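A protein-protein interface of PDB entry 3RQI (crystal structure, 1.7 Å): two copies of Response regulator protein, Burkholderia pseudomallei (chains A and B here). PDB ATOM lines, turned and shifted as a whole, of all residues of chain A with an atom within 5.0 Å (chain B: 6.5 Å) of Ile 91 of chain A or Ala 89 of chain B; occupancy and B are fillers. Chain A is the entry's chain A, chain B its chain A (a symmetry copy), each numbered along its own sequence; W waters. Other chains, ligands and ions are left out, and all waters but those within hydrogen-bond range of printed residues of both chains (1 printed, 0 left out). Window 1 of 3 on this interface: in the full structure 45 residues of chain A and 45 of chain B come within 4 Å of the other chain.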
ATOM      1  N   ALA A  89      -4.888  14.568  30.574  1.00  0.00           N
ATOM      2  CA  ALA A  89      -4.250  13.589  29.696  1.00  0.00           C
ATOM      3  C   ALA A  89      -3.023  14.181  29.006  1.00  0.00           C
ATOM      4  O   ALA A  89      -3.018  15.364  28.622  1.00  0.00           O
ATOM      5  CB  ALA A  89      -5.237  13.034  28.680  1.00  0.00           C
ATOM      6  N   SER A  90      -1.988  13.349  28.869  1.00  0.00           N
ATOM      7  CA  SER A  90      -0.792  13.714  28.115  1.00  0.00           C
ATOM      8  C   SER A  90      -0.069  12.475  27.636  1.00  0.00           C
ATOM      9  O   SER A  90      -0.124  11.402  28.280  1.00  0.00           O
ATOM     10  CB  SER A  90       0.157  14.578  28.959  1.00  0.00           C
ATOM     11  OG  SER A  90       0.599  13.914  30.145  1.00  0.00           O
ATOM     12  N   ILE A  91       0.618  12.617  26.507  1.00  0.00           N
ATOM     13  CA  ILE A  91       1.480  11.491  26.070  1.00  0.00           C
ATOM     14  C   ILE A  91       2.493  11.123  27.130  1.00  0.00           C
ATOM     15  O   ILE A  91       2.711   9.918  27.377  1.00  0.00           O
ATOM     16  CB  ILE A  91       2.134  11.828  24.724  1.00  0.00           C
ATOM     17  CG1 ILE A  91       0.998  11.904  23.698  1.00  0.00           C
ATOM     18  CG2 ILE A  91       3.200  10.802  24.370  1.00  0.00           C
ATOM     19  CD1 ILE A  91       1.430  12.312  22.293  1.00  0.00           C
ATOM     20  N   ALA A  92       3.131  12.109  27.765  1.00  0.00           N
ATOM     21  CA  ALA A  92       4.162  11.765  28.718  1.00  0.00           C
ATOM     22  C   ALA A  92       3.647  10.923  29.890  1.00  0.00           C
ATOM     23  O   ALA A  92       4.295   9.937  30.278  1.00  0.00           O
ATOM     24  CB  ALA A  92       4.894  13.037  29.231  1.00  0.00           C
ATOM     25  N   THR A  93       2.497  11.287  30.440  1.00  0.00           N
ATOM     26  CA  THR A  93       1.977  10.464  31.547  1.00  0.00           C
ATOM     27  C   THR A  93       1.480   9.099  31.092  1.00  0.00           C
ATOM     28  O   THR A  93       1.532   8.139  31.861  1.00  0.00           O
ATOM     29  CB  THR A  93       0.912  11.203  32.335  1.00  0.00           C
ATOM     30  OG1 THR A  93      -0.117  11.640  31.447  1.00  0.00           O
ATOM     31  CG2 THR A  93       1.516  12.370  33.039  1.00  0.00           C
ATOM     32  N   ALA A  94       1.017   9.003  29.846  1.00  0.00           N
ATOM     33  CA  ALA A  94       0.558   7.710  29.312  1.00  0.00           C
ATOM     34  C   ALA A  94       1.761   6.763  29.158  1.00  0.00           C
ATOM     35  O   ALA A  94       1.696   5.634  29.576  1.00  0.00           O
ATOM     36  CB  ALA A  94      -0.181   7.933  27.990  1.00  0.00           C
ATOM     37  N   VAL A  95       2.864   7.265  28.594  1.00  0.00           N
ATOM     38  CA  VAL A  95       4.115   6.479  28.492  1.00  0.00           C
ATOM     39  C   VAL A  95       4.497   5.966  29.893  1.00  0.00           C
ATOM     40  O   VAL A  95       4.706   4.747  30.036  1.00  0.00           O
ATOM     41  CB  VAL A  95       5.259   7.351  27.877  1.00  0.00           C
ATOM     42  CG1 VAL A  95       6.630   6.665  28.026  1.00  0.00           C
ATOM     43  CG2 VAL A  95       4.992   7.666  26.387  1.00  0.00           C
ATOM     44  N   ARG A 171      -0.059  17.454  21.070  1.00  0.00           N
ATOM     45  CA  ARG A 171      -0.916  16.884  20.027  1.00  0.00           C
ATOM     46  C   ARG A 171      -1.676  17.983  19.268  1.00  0.00           C
ATOM     47  O   ARG A 171      -1.787  17.939  18.048  1.00  0.00           O
ATOM     48  CB  ARG A 171      -1.873  15.859  20.632  1.00  0.00           C
ATOM     49  N   GLN A 174       0.712  19.964  16.956  1.00  0.00           N
ATOM     50  CA  GLN A 174       1.005  19.128  15.793  1.00  0.00           C
ATOM     51  C   GLN A 174      -0.150  19.097  14.771  1.00  0.00           C
ATOM     52  O   GLN A 174       0.079  19.118  13.553  1.00  0.00           O
ATOM     53  CB  GLN A 174       1.358  17.702  16.262  1.00  0.00           C
ATOM     54  CG  GLN A 174       2.184  16.896  15.275  1.00  0.00           C
ATOM     55  CD  GLN A 174       2.422  15.476  15.763  1.00  0.00           C
ATOM     56  OE1 GLN A 174       1.477  14.744  16.092  1.00  0.00           O
ATOM     57  NE2 GLN A 174       3.691  15.081  15.813  1.00  0.00           N
ATOM     58  N   LEU B  59       6.102   6.070  12.958  1.00  0.00           N
ATOM     59  CA  LEU B  59       4.939   5.183  12.983  1.00  0.00           C
ATOM     60  C   LEU B  59       4.345   4.941  11.613  1.00  0.00           C
ATOM     61  O   LEU B  59       4.044   3.798  11.247  1.00  0.00           O
ATOM     62  CB  LEU B  59       3.833   5.728  13.917  1.00  0.00           C
ATOM     63  CG  LEU B  59       4.270   5.779  15.380  1.00  0.00           C
ATOM     64  CD1 LEU B  59       3.149   6.357  16.248  1.00  0.00           C
ATOM     65  CD2 LEU B  59       4.736   4.397  15.887  1.00  0.00           C
ATOM     66  N   THR B  86       7.347  10.732  15.890  1.00  0.00           N
ATOM     67  CA  THR B  86       6.191  10.668  14.941  1.00  0.00           C
ATOM     68  C   THR B  86       5.455  11.974  14.708  1.00  0.00           C
ATOM     69  O   THR B  86       5.233  12.750  15.645  1.00  0.00           O
ATOM     70  CB  THR B  86       5.155   9.570  15.356  1.00  0.00           C
ATOM     71  OG1 THR B  86       4.070   9.509  14.446  1.00  0.00           O
ATOM     72  CG2 THR B  86       4.618   9.797  16.731  1.00  0.00           C
ATOM     73  N   GLY B  87       5.067  12.189  13.453  1.00  0.00           N
ATOM     74  CA  GLY B  87       4.194  13.313  13.078  1.00  0.00           C
ATOM     75  C   GLY B  87       2.710  12.975  13.242  1.00  0.00           C
ATOM     76  O   GLY B  87       1.838  13.803  12.945  1.00  0.00           O
ATOM     77  N   TYR B  88       2.433  11.758  13.727  1.00  0.00           N
ATOM     78  CA  TYR B  88       1.080  11.311  13.978  1.00  0.00           C
ATOM     79  C   TYR B  88       0.853  10.941  15.446  1.00  0.00           C
ATOM     80  O   TYR B  88       0.440   9.833  15.766  1.00  0.00           O
ATOM     81  CB  TYR B  88       0.740  10.164  13.049  1.00  0.00           C
ATOM     82  CG  TYR B  88       0.812  10.582  11.605  1.00  0.00           C
ATOM     83  CD1 TYR B  88      -0.196  11.357  11.016  1.00  0.00           C
ATOM     84  CD2 TYR B  88       1.921  10.254  10.845  1.00  0.00           C
ATOM     85  CE1 TYR B  88      -0.098  11.752   9.676  1.00  0.00           C
ATOM     86  CE2 TYR B  88       2.024  10.637   9.535  1.00  0.00           C
ATOM     87  CZ  TYR B  88       1.026  11.382   8.944  1.00  0.00           C
ATOM     88  OH  TYR B  88       1.167  11.734   7.612  1.00  0.00           O
ATOM     89  N   ALA B  89       1.163  11.869  16.346  1.00  0.00           N
ATOM     90  CA  ALA B  89       1.188  11.504  17.761  1.00  0.00           C
ATOM     91  C   ALA B  89      -0.223  11.286  18.302  1.00  0.00           C
ATOM     92  O   ALA B  89      -1.166  12.004  17.926  1.00  0.00           O
ATOM     93  CB  ALA B  89       1.938  12.540  18.584  1.00  0.00           C
ATOM     94  N   SER B  90      -0.353  10.282  19.172  1.00  0.00           N
ATOM     95  CA  SER B  90      -1.602  10.025  19.883  1.00  0.00           C
ATOM     96  C   SER B  90      -1.338   9.262  21.161  1.00  0.00           C
ATOM     97  O   SER B  90      -0.366   8.478  21.259  1.00  0.00           O
ATOM     98  CB  SER B  90      -2.593   9.245  19.005  1.00  0.00           C
ATOM     99  OG  SER B  90      -2.081   7.976  18.591  1.00  0.00           O
ATOM    100  N   ILE B  91      -2.203   9.482  22.146  1.00  0.00           N
ATOM    101  CA  ILE B  91      -2.097   8.646  23.367  1.00  0.00           C
ATOM    102  C   ILE B  91      -2.202   7.173  23.042  1.00  0.00           C
ATOM    103  O   ILE B  91      -1.429   6.367  23.599  1.00  0.00           O
ATOM    104  CB  ILE B  91      -3.140   9.097  24.398  1.00  0.00           C
ATOM    105  CG1 ILE B  91      -2.740  10.512  24.828  1.00  0.00           C
ATOM    106  CG2 ILE B  91      -3.214   8.112  25.555  1.00  0.00           C
ATOM    107  CD1 ILE B  91      -3.703  11.182  25.803  1.00  0.00           C
ATOM    108  N   THR B  93      -1.390   5.355  20.393  1.00  0.00           N
ATOM    109  CA  THR B  93      -0.161   4.740  19.860  1.00  0.00           C
ATOM    110  C   THR B  93       0.996   4.768  20.849  1.00  0.00           C
ATOM    111  O   THR B  93       1.853   3.885  20.817  1.00  0.00           O
ATOM    112  CB  THR B  93       0.236   5.355  18.531  1.00  0.00           C
ATOM    113  OG1 THR B  93       0.351   6.770  18.680  1.00  0.00           O
ATOM    114  CG2 THR B  93      -0.782   5.026  17.493  1.00  0.00           C
ATOM    115  N   ALA B  94       1.015   5.763  21.737  1.00  0.00           N
ATOM    116  CA  ALA B  94       2.074   5.839  22.756  1.00  0.00           C
ATOM    117  C   ALA B  94       1.911   4.678  23.752  1.00  0.00           C
ATOM    118  O   ALA B  94       2.865   4.005  24.054  1.00  0.00           O
ATOM    119  CB  ALA B  94       2.029   7.207  23.443  1.00  0.00           C
ATOM    120  N   TYR B 105       8.659   8.253  23.663  1.00  0.00           N
ATOM    121  CA  TYR B 105       7.827   8.593  22.507  1.00  0.00           C
ATOM    122  C   TYR B 105       7.822  10.099  22.430  1.00  0.00           C
ATOM    123  O   TYR B 105       7.617  10.772  23.440  1.00  0.00           O
ATOM    124  CB  TYR B 105       6.424   8.023  22.758  1.00  0.00           C
ATOM    125  CG  TYR B 105       5.326   8.216  21.699  1.00  0.00           C
ATOM    126  CD1 TYR B 105       4.781   7.100  21.053  1.00  0.00           C
ATOM    127  CD2 TYR B 105       4.822   9.507  21.391  1.00  0.00           C
ATOM    128  CE1 TYR B 105       3.732   7.227  20.137  1.00  0.00           C
ATOM    129  CE2 TYR B 105       3.789   9.657  20.472  1.00  0.00           C
ATOM    130  CZ  TYR B 105       3.246   8.514  19.862  1.00  0.00           C
ATOM    131  OH  TYR B 105       2.230   8.660  18.971  1.00  0.00           O
ATOM    132  N   LEU B 106       8.129  10.637  21.252  1.00  0.00           N
ATOM    133  CA  LEU B 106       8.144  12.098  21.024  1.00  0.00           C
ATOM    134  C   LEU B 106       7.408  12.485  19.757  1.00  0.00           C
ATOM    135  O   LEU B 106       7.497  11.805  18.716  1.00  0.00           O
ATOM    136  CB  LEU B 106       9.576  12.588  20.871  1.00  0.00           C
ATOM    137  CG  LEU B 106      10.471  12.922  22.057  1.00  0.00           C
ATOM    138  CD1 LEU B 106      11.663  13.675  21.420  1.00  0.00           C
ATOM    139  CD2 LEU B 106       9.738  13.783  23.081  1.00  0.00           C
ATOM    140  N   ALA B 107       6.630  13.567  19.863  1.00  0.00           N
ATOM    141  CA  ALA B 107       6.033  14.182  18.669  1.00  0.00           C
ATOM    142  C   ALA B 107       7.042  14.978  17.849  1.00  0.00           C
ATOM    143  O   ALA B 107       7.863  15.739  18.412  1.00  0.00           O
ATOM    144  CB  ALA B 107       4.864  15.091  19.078  1.00  0.00           C
ATOM    145  N   LYS B 108       6.995  14.796  16.520  1.00  0.00           N
ATOM    146  CA  LYS B 108       7.613  15.744  15.600  1.00  0.00           C
ATOM    147  C   LYS B 108       6.816  17.081  15.635  1.00  0.00           C
ATOM    148  O   LYS B 108       5.589  17.079  15.853  1.00  0.00           O
ATOM    149  CB  LYS B 108       7.648  15.228  14.156  1.00  0.00           C
ATOM    150  CG  LYS B 108       8.436  13.949  13.910  1.00  0.00           C
ATOM    151  CD  LYS B 108       8.296  13.543  12.445  1.00  0.00           C
ATOM    152  CE  LYS B 108       9.078  12.243  12.152  1.00  0.00           C
ATOM    153  NZ  LYS B 108       8.594  11.718  10.848  1.00  0.00           N
ATOM    154  N   HIS B 169      -7.628  15.987  18.173  1.00  0.00           N
ATOM    155  CA  HIS B 169      -7.036  15.102  19.178  1.00  0.00           C
ATOM    156  C   HIS B 169      -7.861  15.109  20.457  1.00  0.00           C
ATOM    157  O   HIS B 169      -8.503  16.113  20.802  1.00  0.00           O
ATOM    158  CB  HIS B 169      -5.596  15.498  19.470  1.00  0.00           C
ATOM    159  CG  HIS B 169      -4.673  15.281  18.323  1.00  0.00           C
ATOM    160  ND1 HIS B 169      -4.047  14.076  18.091  1.00  0.00           N
ATOM    161  CD2 HIS B 169      -4.262  16.117  17.341  1.00  0.00           C
ATOM    162  CE1 HIS B 169      -3.292  14.180  17.014  1.00  0.00           C
ATOM    163  NE2 HIS B 169      -3.399  15.409  16.545  1.00  0.00           N
HETATM  164  O   HOH W   1      -0.681  14.871  13.595  1.00  0.00           O
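NE2 of His 169 of chain B sits close to O of Arg 171 of chain A, at 3.4 Å.
The side-chain amide nitrogen of Gln 174 of chain A sits at hydrogen-bond distance from the backbone carbonyl oxygen of Thr 86 of chain B (2.8 Å).
O of Gly 87 of chain B lies close to OE1 of Gln 174 of chain A, at 3.3 Å.
N of Ala 89 of chain B sits at hydrogen-bond distance from OE1 of Gln 174 of chain A.
The side-chain amide nitrogen of Gln 174 of chain A is in hydrogen-bond range of the backbone carbonyl oxygen of Lys 108 of chain B.
The backbone NH of Tyr 88 of chain B sits at hydrogen-bond distance from the side-chain hydroxyl of Thr 86 of chain B (2.9 Å).
The backbone carbonyl oxygen (O) of Leu 106 of chain B sits at hydrogen-bond distance from the backbone NH (N) of Thr 86 of chain B, 3.0 Å away.
O of Thr 86 of chain B is in hydrogen-bond range of N of Lys 108 of chain B, at 2.8 Å.
N of Ser 90 of chain B is in hydrogen-bond range of OH of Tyr 105 of chain B, at 3.1 Å.
OH of Tyr 105 of chain B sits at hydrogen-bond distance from OG1 of Thr 93 of chain B, 2.7 Å away.
Among the printed residues, merely in contact across the chains: Gln 174 of chain A with Ala 107 of chain B, Ile 91 of chain A with Tyr 105 of chain B, Ala 89 of chain A with Ile 91 of chain B, Ile 91 of chain A with Ala 89 of chain B, Ile 91 of chain A with Ala 94 of chain B, Ala 94 of chain A with Ile 91 of chain B, Gln 174 of chain A with Tyr 88 of chain B and Val 95 of chain A with Tyr 105 of chain B.
Ser 90 of chain A touches none of the printed residues of chain B.
Printed residues of chain A within 4 Å of Tyr 88 of chain B: Gln 174 (3.9 Å).
Of chain A, only Ile 91 (3.8 Å) and Gln 174 (2.9 Å) come within 4 Å of Ala 89 of chain B.
Printed residues of chain A within 4 Å of Lys 108 of chain B: Gln 174 (2.8 Å).
Of the printed residues of chain A, His 169 of chain B touches Arg 171 (3.2 Å).
The nearest printed residue of chain B that does not touch Ile 91 of chain A is Ser 90 of chain B (4.1 Å).
The nearest printed residue of chain A that does not touch Gly 87 of chain B is Arg 171 of chain A (7.5 Å).
Along chain B the printed residues that touch a printed residue of chain A span positions 86 to 169.
Hydrophobic or aromatic side chains of chain A that line the printed part of chain B: Ala 89, Ile 91, Ala 94 and Val 95.
Along chain A the printed residues that touch a printed residue of chain B span positions 89 to 174.
Among the printed residues, no Asp or Glu carboxylate lies within 4 Å of a Lys or Arg side-chain nitrogen of the other chain.
Ala 89 of chain A touches Ile 91 of chain B, and with the chains exchanged Ile 91 of chain A touches Ala 89 of chain B.
Ile 91 of chain A touches Ala 94 of chain B, and with the chains exchanged Ala 94 of chain A touches Ile 91 of chain B.
Positions printed for both chains: 89, 90, 91, 93 and 94.
Water W1 lies within hydrogen-bond range of O of Gly 87 of chain B (2.8 Å) and OE1 of Gln 174 of chain A (3.3 Å).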
